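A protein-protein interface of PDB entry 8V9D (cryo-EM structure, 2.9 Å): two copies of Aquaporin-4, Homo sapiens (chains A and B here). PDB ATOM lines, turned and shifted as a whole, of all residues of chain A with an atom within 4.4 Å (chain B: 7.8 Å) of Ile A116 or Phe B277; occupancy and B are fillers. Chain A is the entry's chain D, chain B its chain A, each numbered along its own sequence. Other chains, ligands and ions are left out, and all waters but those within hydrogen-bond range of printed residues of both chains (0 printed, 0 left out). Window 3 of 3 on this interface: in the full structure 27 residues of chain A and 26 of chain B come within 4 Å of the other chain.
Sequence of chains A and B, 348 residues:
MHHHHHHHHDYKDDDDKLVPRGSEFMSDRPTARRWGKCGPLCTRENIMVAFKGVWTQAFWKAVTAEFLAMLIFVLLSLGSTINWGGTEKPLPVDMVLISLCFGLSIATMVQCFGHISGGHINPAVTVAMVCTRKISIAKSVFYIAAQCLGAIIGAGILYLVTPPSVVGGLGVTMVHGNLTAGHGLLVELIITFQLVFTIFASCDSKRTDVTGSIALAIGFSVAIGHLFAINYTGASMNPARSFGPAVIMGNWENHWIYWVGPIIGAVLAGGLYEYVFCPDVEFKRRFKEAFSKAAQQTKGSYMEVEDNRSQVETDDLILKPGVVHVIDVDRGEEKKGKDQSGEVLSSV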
ATOM      1  N   LYS A  61       6.950   8.235 -25.478  1.00  0.00           N
ATOM      2  CA  LYS A  61       7.740   8.811 -24.397  1.00  0.00           C
ATOM      3  C   LYS A  61       7.104  10.083 -23.859  1.00  0.00           C
ATOM      4  O   LYS A  61       7.191  10.356 -22.658  1.00  0.00           O
ATOM      5  CB  LYS A  61       9.160   9.095 -24.878  1.00  0.00           C
ATOM      6  CG  LYS A  61       9.976   7.858 -25.182  1.00  0.00           C
ATOM      7  CD  LYS A  61      11.381   8.231 -25.620  1.00  0.00           C
ATOM      8  CE  LYS A  61      12.203   7.000 -25.948  1.00  0.00           C
ATOM      9  NZ  LYS A  61      13.576   7.356 -26.392  1.00  0.00           N
ATOM     10  N   ALA A  62       6.470  10.874 -24.727  1.00  0.00           N
ATOM     11  CA  ALA A  62       5.794  12.084 -24.271  1.00  0.00           C
ATOM     12  C   ALA A  62       4.537  11.750 -23.480  1.00  0.00           C
ATOM     13  O   ALA A  62       4.211  12.434 -22.505  1.00  0.00           O
ATOM     14  CB  ALA A  62       5.457  12.977 -25.462  1.00  0.00           C
ATOM     15  N   THR A  64       4.095   8.983 -21.738  1.00  0.00           N
ATOM     16  CA  THR A  64       4.542   8.425 -20.468  1.00  0.00           C
ATOM     17  C   THR A  64       5.030   9.508 -19.516  1.00  0.00           C
ATOM     18  O   THR A  64       4.858   9.386 -18.299  1.00  0.00           O
ATOM     19  CB  THR A  64       5.644   7.395 -20.707  1.00  0.00           C
ATOM     20  OG1 THR A  64       5.144   6.346 -21.542  1.00  0.00           O
ATOM     21  CG2 THR A  64       6.117   6.806 -19.393  1.00  0.00           C
ATOM     22  N   ALA A  65       5.651  10.564 -20.045  1.00  0.00           N
ATOM     23  CA  ALA A  65       6.096  11.665 -19.197  1.00  0.00           C
ATOM     24  C   ALA A  65       4.913  12.421 -18.605  1.00  0.00           C
ATOM     25  O   ALA A  65       4.979  12.890 -17.463  1.00  0.00           O
ATOM     26  CB  ALA A  65       6.993  12.610 -19.993  1.00  0.00           C
ATOM     27  N   CYS A 112      11.844  18.988 -15.163  1.00  0.00           N
ATOM     28  CA  CYS A 112      12.189  17.590 -15.396  1.00  0.00           C
ATOM     29  C   CYS A 112      11.739  17.125 -16.775  1.00  0.00           C
ATOM     30  O   CYS A 112      12.517  16.523 -17.523  1.00  0.00           O
ATOM     31  CB  CYS A 112      11.562  16.714 -14.313  1.00  0.00           C
ATOM     32  SG  CYS A 112      12.376  16.783 -12.715  1.00  0.00           S
ATOM     33  N   PHE A 113      10.486  17.402 -17.132  1.00  0.00           N
ATOM     34  CA  PHE A 113       9.852  16.813 -18.304  1.00  0.00           C
ATOM     35  C   PHE A 113       9.557  17.830 -19.398  1.00  0.00           C
ATOM     36  O   PHE A 113       8.904  17.485 -20.387  1.00  0.00           O
ATOM     37  CB  PHE A 113       8.561  16.103 -17.891  1.00  0.00           C
ATOM     38  CG  PHE A 113       8.783  14.902 -17.015  1.00  0.00           C
ATOM     39  CD1 PHE A 113       9.259  13.718 -17.546  1.00  0.00           C
ATOM     40  CD2 PHE A 113       8.528  14.963 -15.658  1.00  0.00           C
ATOM     41  CE1 PHE A 113       9.463  12.619 -16.743  1.00  0.00           C
ATOM     42  CE2 PHE A 113       8.734  13.866 -14.852  1.00  0.00           C
ATOM     43  CZ  PHE A 113       9.201  12.693 -15.395  1.00  0.00           C
ATOM     44  N   GLY A 114      10.026  19.067 -19.255  1.00  0.00           N
ATOM     45  CA  GLY A 114       9.688  20.091 -20.230  1.00  0.00           C
ATOM     46  C   GLY A 114      10.175  19.765 -21.628  1.00  0.00           C
ATOM     47  O   GLY A 114       9.519  20.098 -22.616  1.00  0.00           O
ATOM     48  N   HIS A 115      11.334  19.125 -21.733  1.00  0.00           N
ATOM     49  CA  HIS A 115      11.923  18.789 -23.021  1.00  0.00           C
ATOM     50  C   HIS A 115      11.465  17.441 -23.560  1.00  0.00           C
ATOM     51  O   HIS A 115      11.817  17.093 -24.691  1.00  0.00           O
ATOM     52  CB  HIS A 115      13.451  18.807 -22.917  1.00  0.00           C
ATOM     53  CG  HIS A 115      14.006  17.766 -21.996  1.00  0.00           C
ATOM     54  ND1 HIS A 115      13.575  17.617 -20.696  1.00  0.00           N
ATOM     55  CD2 HIS A 115      14.959  16.825 -22.186  1.00  0.00           C
ATOM     56  CE1 HIS A 115      14.238  16.629 -20.126  1.00  0.00           C
ATOM     57  NE2 HIS A 115      15.083  16.130 -21.008  1.00  0.00           N
ATOM     58  N   ILE A 116      10.693  16.680 -22.792  1.00  0.00           N
ATOM     59  CA  ILE A 116      10.250  15.358 -23.206  1.00  0.00           C
ATOM     60  C   ILE A 116       8.821  15.384 -23.734  1.00  0.00           C
ATOM     61  O   ILE A 116       8.527  14.773 -24.760  1.00  0.00           O
ATOM     62  CB  ILE A 116      10.390  14.357 -22.041  1.00  0.00           C
ATOM     63  CG1 ILE A 116      11.835  14.303 -21.551  1.00  0.00           C
ATOM     64  CG2 ILE A 116       9.944  12.976 -22.475  1.00  0.00           C
ATOM     65  CD1 ILE A 116      12.014  13.515 -20.282  1.00  0.00           C
ATOM     66  N   SER A 117       7.924  16.086 -23.044  1.00  0.00           N
ATOM     67  CA  SER A 117       6.517  16.111 -23.407  1.00  0.00           C
ATOM     68  C   SER A 117       5.956  17.506 -23.628  1.00  0.00           C
ATOM     69  O   SER A 117       4.825  17.624 -24.112  1.00  0.00           O
ATOM     70  CB  SER A 117       5.677  15.416 -22.327  1.00  0.00           C
ATOM     71  OG  SER A 117       5.653  16.181 -21.138  1.00  0.00           O
ATOM     72  N   GLY A 118       6.699  18.557 -23.297  1.00  0.00           N
ATOM     73  CA  GLY A 118       6.187  19.907 -23.326  1.00  0.00           C
ATOM     74  C   GLY A 118       5.808  20.463 -21.971  1.00  0.00           C
ATOM     75  O   GLY A 118       5.598  21.676 -21.856  1.00  0.00           O
ATOM     76  N   PHE B 193      13.176   9.731  -5.864  1.00  0.00           N
ATOM     77  CA  PHE B 193      13.136   9.499  -7.302  1.00  0.00           C
ATOM     78  C   PHE B 193      13.066  10.812  -8.069  1.00  0.00           C
ATOM     79  O   PHE B 193      13.774  10.995  -9.065  1.00  0.00           O
ATOM     80  CB  PHE B 193      11.945   8.605  -7.655  1.00  0.00           C
ATOM     81  CG  PHE B 193      11.712   8.458  -9.132  1.00  0.00           C
ATOM     82  CD1 PHE B 193      10.889   9.339  -9.809  1.00  0.00           C
ATOM     83  CD2 PHE B 193      12.314   7.440  -9.843  1.00  0.00           C
ATOM     84  CE1 PHE B 193      10.678   9.208 -11.163  1.00  0.00           C
ATOM     85  CE2 PHE B 193      12.104   7.306 -11.197  1.00  0.00           C
ATOM     86  CZ  PHE B 193      11.286   8.191 -11.858  1.00  0.00           C
ATOM     87  N   PHE B 197      15.987  12.647 -10.621  1.00  0.00           N
ATOM     88  CA  PHE B 197      15.553  12.960 -11.977  1.00  0.00           C
ATOM     89  C   PHE B 197      15.783  14.431 -12.292  1.00  0.00           C
ATOM     90  O   PHE B 197      16.143  14.783 -13.420  1.00  0.00           O
ATOM     91  CB  PHE B 197      14.079  12.590 -12.150  1.00  0.00           C
ATOM     92  CG  PHE B 197      13.696  12.247 -13.564  1.00  0.00           C
ATOM     93  CD1 PHE B 197      13.440  13.243 -14.488  1.00  0.00           C
ATOM     94  CD2 PHE B 197      13.584  10.927 -13.961  1.00  0.00           C
ATOM     95  CE1 PHE B 197      13.089  12.928 -15.783  1.00  0.00           C
ATOM     96  CE2 PHE B 197      13.233  10.607 -15.254  1.00  0.00           C
ATOM     97  CZ  PHE B 197      12.985  11.609 -16.166  1.00  0.00           C
ATOM     98  N   ALA B 201      18.274  15.822 -15.210  1.00  0.00           N
ATOM     99  CA  ALA B 201      17.680  16.659 -16.247  1.00  0.00           C
ATOM    100  C   ALA B 201      18.326  18.039 -16.291  1.00  0.00           C
ATOM    101  O   ALA B 201      18.589  18.570 -17.375  1.00  0.00           O
ATOM    102  CB  ALA B 201      16.175  16.779 -16.020  1.00  0.00           C
ATOM    103  N   LYS B 206      23.134  17.548 -23.282  1.00  0.00           N
ATOM    104  CA  LYS B 206      22.485  17.573 -24.586  1.00  0.00           C
ATOM    105  C   LYS B 206      21.358  18.594 -24.663  1.00  0.00           C
ATOM    106  O   LYS B 206      20.962  18.975 -25.768  1.00  0.00           O
ATOM    107  CB  LYS B 206      21.944  16.185 -24.927  1.00  0.00           C
ATOM    108  CG  LYS B 206      23.017  15.120 -25.065  1.00  0.00           C
ATOM    109  CD  LYS B 206      22.421  13.786 -25.483  1.00  0.00           C
ATOM    110  CE  LYS B 206      21.602  13.169 -24.363  1.00  0.00           C
ATOM    111  NZ  LYS B 206      22.445  12.789 -23.201  1.00  0.00           N
ATOM    112  N   ARG B 207      20.836  19.040 -23.525  1.00  0.00           N
ATOM    113  CA  ARG B 207      19.743  20.000 -23.525  1.00  0.00           C
ATOM    114  C   ARG B 207      20.228  21.376 -23.957  1.00  0.00           C
ATOM    115  O   ARG B 207      21.371  21.767 -23.709  1.00  0.00           O
ATOM    116  CB  ARG B 207      19.109  20.094 -22.136  1.00  0.00           C
ATOM    117  CG  ARG B 207      18.302  18.883 -21.724  1.00  0.00           C
ATOM    118  CD  ARG B 207      17.609  19.106 -20.391  1.00  0.00           C
ATOM    119  NE  ARG B 207      16.525  20.078 -20.470  1.00  0.00           N
ATOM    120  CZ  ARG B 207      15.685  20.341 -19.479  1.00  0.00           C
ATOM    121  NH1 ARG B 207      15.786  19.737 -18.308  1.00  0.00           N
ATOM    122  NH2 ARG B 207      14.714  21.229 -19.669  1.00  0.00           N
ATOM    123  N   ASP B 209      17.516  23.907 -23.678  1.00  0.00           N
ATOM    124  CA  ASP B 209      16.382  24.684 -23.196  1.00  0.00           C
ATOM    125  C   ASP B 209      16.415  24.913 -21.692  1.00  0.00           C
ATOM    126  O   ASP B 209      15.429  25.403 -21.131  1.00  0.00           O
ATOM    127  CB  ASP B 209      15.075  23.997 -23.585  1.00  0.00           C
ATOM    128  CG  ASP B 209      14.988  22.580 -23.067  1.00  0.00           C
ATOM    129  OD1 ASP B 209      15.794  21.736 -23.506  1.00  0.00           O
ATOM    130  OD2 ASP B 209      14.113  22.309 -22.219  1.00  0.00           O
ATOM    131  N   LEU B 268      16.683   4.094  -9.978  1.00  0.00           N
ATOM    132  CA  LEU B 268      15.577   4.081 -10.929  1.00  0.00           C
ATOM    133  C   LEU B 268      15.528   5.378 -11.725  1.00  0.00           C
ATOM    134  O   LEU B 268      15.363   5.365 -12.950  1.00  0.00           O
ATOM    135  CB  LEU B 268      14.255   3.853 -10.199  1.00  0.00           C
ATOM    136  CG  LEU B 268      14.030   2.506  -9.515  1.00  0.00           C
ATOM    137  CD1 LEU B 268      12.728   2.534  -8.740  1.00  0.00           C
ATOM    138  CD2 LEU B 268      14.023   1.379 -10.530  1.00  0.00           C
ATOM    139  N   ALA B 269      15.664   6.516 -11.042  1.00  0.00           N
ATOM    140  CA  ALA B 269      15.638   7.802 -11.729  1.00  0.00           C
ATOM    141  C   ALA B 269      16.832   7.959 -12.661  1.00  0.00           C
ATOM    142  O   ALA B 269      16.687   8.437 -13.791  1.00  0.00           O
ATOM    143  CB  ALA B 269      15.600   8.940 -10.712  1.00  0.00           C
ATOM    144  N   GLY B 271      18.783   5.514 -14.025  1.00  0.00           N
ATOM    145  CA  GLY B 271      18.685   4.577 -15.131  1.00  0.00           C
ATOM    146  C   GLY B 271      17.537   4.890 -16.071  1.00  0.00           C
ATOM    147  O   GLY B 271      17.665   4.756 -17.290  1.00  0.00           O
ATOM    148  N   LEU B 272      16.395   5.299 -15.518  1.00  0.00           N
ATOM    149  CA  LEU B 272      15.228   5.587 -16.346  1.00  0.00           C
ATOM    150  C   LEU B 272      15.475   6.790 -17.250  1.00  0.00           C
ATOM    151  O   LEU B 272      15.096   6.776 -18.425  1.00  0.00           O
ATOM    152  CB  LEU B 272      14.010   5.812 -15.453  1.00  0.00           C
ATOM    153  CG  LEU B 272      12.646   6.050 -16.096  1.00  0.00           C
ATOM    154  CD1 LEU B 272      12.223   4.836 -16.899  1.00  0.00           C
ATOM    155  CD2 LEU B 272      11.616   6.370 -15.031  1.00  0.00           C
ATOM    156  N   TYR B 273      16.098   7.842 -16.717  1.00  0.00           N
ATOM    157  CA  TYR B 273      16.454   8.994 -17.539  1.00  0.00           C
ATOM    158  C   TYR B 273      17.544   8.646 -18.543  1.00  0.00           C
ATOM    159  O   TYR B 273      17.415   8.923 -19.740  1.00  0.00           O
ATOM    160  CB  TYR B 273      16.915  10.150 -16.653  1.00  0.00           C
ATOM    161  CG  TYR B 273      17.139  11.441 -17.409  1.00  0.00           C
ATOM    162  CD1 TYR B 273      16.114  12.353 -17.590  1.00  0.00           C
ATOM    163  CD2 TYR B 273      18.372  11.725 -17.970  1.00  0.00           C
ATOM    164  CE1 TYR B 273      16.319  13.521 -18.288  1.00  0.00           C
ATOM    165  CE2 TYR B 273      18.584  12.888 -18.672  1.00  0.00           C
ATOM    166  CZ  TYR B 273      17.555  13.783 -18.828  1.00  0.00           C
ATOM    167  OH  TYR B 273      17.769  14.945 -19.529  1.00  0.00           O
ATOM    168  N   GLU B 274      18.626   8.031 -18.070  1.00  0.00           N
ATOM    169  CA  GLU B 274      19.830   7.910 -18.881  1.00  0.00           C
ATOM    170  C   GLU B 274      19.677   6.881 -19.993  1.00  0.00           C
ATOM    171  O   GLU B 274      20.415   6.932 -20.983  1.00  0.00           O
ATOM    172  CB  GLU B 274      21.014   7.552 -17.986  1.00  0.00           C
ATOM    173  CG  GLU B 274      22.336   7.445 -18.710  1.00  0.00           C
ATOM    174  CD  GLU B 274      22.787   8.767 -19.283  1.00  0.00           C
ATOM    175  OE1 GLU B 274      22.381   9.816 -18.744  1.00  0.00           O
ATOM    176  OE2 GLU B 274      23.546   8.758 -20.273  1.00  0.00           O
ATOM    177  N   TYR B 275      18.743   5.942 -19.854  1.00  0.00           N
ATOM    178  CA  TYR B 275      18.670   4.802 -20.753  1.00  0.00           C
ATOM    179  C   TYR B 275      17.336   4.653 -21.470  1.00  0.00           C
ATOM    180  O   TYR B 275      17.251   3.856 -22.409  1.00  0.00           O
ATOM    181  CB  TYR B 275      18.964   3.507 -19.980  1.00  0.00           C
ATOM    182  CG  TYR B 275      20.386   3.419 -19.480  1.00  0.00           C
ATOM    183  CD1 TYR B 275      21.451   3.801 -20.284  1.00  0.00           C
ATOM    184  CD2 TYR B 275      20.663   2.987 -18.193  1.00  0.00           C
ATOM    185  CE1 TYR B 275      22.750   3.732 -19.825  1.00  0.00           C
ATOM    186  CE2 TYR B 275      21.958   2.919 -17.726  1.00  0.00           C
ATOM    187  CZ  TYR B 275      22.995   3.292 -18.546  1.00  0.00           C
ATOM    188  OH  TYR B 275      24.287   3.222 -18.085  1.00  0.00           O
ATOM    189  N   VAL B 276      16.301   5.389 -21.068  1.00  0.00           N
ATOM    190  CA  VAL B 276      14.965   5.255 -21.635  1.00  0.00           C
ATOM    191  C   VAL B 276      14.480   6.567 -22.240  1.00  0.00           C
ATOM    192  O   VAL B 276      14.063   6.610 -23.400  1.00  0.00           O
ATOM    193  CB  VAL B 276      13.958   4.736 -20.586  1.00  0.00           C
ATOM    194  CG1 VAL B 276      12.570   4.652 -21.183  1.00  0.00           C
ATOM    195  CG2 VAL B 276      14.393   3.381 -20.063  1.00  0.00           C
ATOM    196  N   PHE B 277      14.529   7.652 -21.467  1.00  0.00           N
ATOM    197  CA  PHE B 277      13.963   8.912 -21.933  1.00  0.00           C
ATOM    198  C   PHE B 277      14.926   9.658 -22.848  1.00  0.00           C
ATOM    199  O   PHE B 277      14.568  10.014 -23.976  1.00  0.00           O
ATOM    200  CB  PHE B 277      13.574   9.788 -20.740  1.00  0.00           C
ATOM    201  CG  PHE B 277      12.249   9.430 -20.136  1.00  0.00           C
ATOM    202  CD1 PHE B 277      11.085   9.541 -20.874  1.00  0.00           C
ATOM    203  CD2 PHE B 277      12.165   8.989 -18.829  1.00  0.00           C
ATOM    204  CE1 PHE B 277       9.867   9.213 -20.321  1.00  0.00           C
ATOM    205  CE2 PHE B 277      10.947   8.659 -18.272  1.00  0.00           C
ATOM    206  CZ  PHE B 277       9.798   8.773 -19.019  1.00  0.00           C
ATOM    207  N   CYS B 278      16.147   9.906 -22.383  1.00  0.00           N
ATOM    208  CA  CYS B 278      17.138  10.681 -23.129  1.00  0.00           C
ATOM    209  C   CYS B 278      18.439   9.895 -23.203  1.00  0.00           C
ATOM    210  O   CYS B 278      19.426  10.232 -22.539  1.00  0.00           O
ATOM    211  CB  CYS B 278      17.360  12.050 -22.486  1.00  0.00           C
ATOM    212  SG  CYS B 278      15.863  13.036 -22.300  1.00  0.00           S
ATOM    213  N   PRO B 279      18.475   8.831 -24.018  1.00  0.00           N
ATOM    214  CA  PRO B 279      19.650   7.974 -24.182  1.00  0.00           C
ATOM    215  C   PRO B 279      20.722   8.601 -25.067  1.00  0.00           C
ATOM    216  O   PRO B 279      20.393   9.106 -26.138  1.00  0.00           O
ATOM    217  CB  PRO B 279      19.070   6.720 -24.833  1.00  0.00           C
ATOM    218  CG  PRO B 279      17.927   7.225 -25.624  1.00  0.00           C
ATOM    219  CD  PRO B 279      17.348   8.380 -24.851  1.00  0.00           C
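The side-chain hydroxyl of Tyr B273 is in hydrogen-bond range of a ring nitrogen (NE2) of His A115 (3.3 Å). O of Val B276 is in hydrogen-bond range of NZ of Lys A61. The side-chain sulfur (SG) of Cys B278 lies within hydrogen-bond range of a ring nitrogen (NE2) of His A115 (3.4 Å).
NH1 of Arg B207 is in hydrogen-bond range of O of Ala B201, 3.2 Å away. The guanidinium group (NH2) of Arg B207 is in salt-bridge range of the side-chain carboxylate (OD2) of Asp B209. The backbone carbonyl oxygen (O) of Leu B272 lies within hydrogen-bond range of the backbone NH (N) of Phe B277 (3.2 Å). The backbone carbonyl oxygen (O) of Tyr B273 is in hydrogen-bond range of the backbone NH (N) of Cys B278 (3.1 Å).
Lys A61 touches Phe B277. Phe B197 touches Cys A112 (CD1 to CB, 3.95 Å). O of Cys A112 touches CB of Ala B201, 3.96 Å away. Phe A113 touches Phe B197. CZ of Arg B207 touches ND1 of His A115, at 3.7 Å. His A115 touches Asp B209. Ile A116 touches Phe B277 (CG2 to CD1, 3.96 Å).
Printed residues of chain A within 4 Å of Phe B197: Cys A112 (3.95 Å) and Phe A113 (3.7 Å). Printed residues of chain A within 4 Å of Ala B201: Cys A112 (3.96 Å). Of the printed residues of chain A, Val B276 touches Lys A61. Of the printed residues of chain A, Arg B207 touches His A115. Of the printed residues of chain A, Tyr B273 touches His A115 (3.3 Å). Pro B279 touches none of the printed residues of chain A. Tyr B275 touches none of the printed residues of chain A. The nearest printed residue of chain A that does not touch Val B276 is Thr A64 (7.0 Å).
Of the 11 printed residues of chain A, 5 touch a printed residue of chain B. Hydrophobic or aromatic side chains of chain A that line the printed part of chain B: Phe A113, His A115 and Ile A116. Of the 17 printed residues of chain B, 8 touch a printed residue of chain A. Hydrophobic or aromatic side chains of chain B within 4 Å of the printed part of chain A: Phe B197, Ala B201, Tyr B273 and Phe B277. Among the printed residues, 10 pairs touch across the chains.
No position is printed for both chains. Of the 10 pairs that touch across the chains among the printed residues, none has its exchanged pair printed and touching as well.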
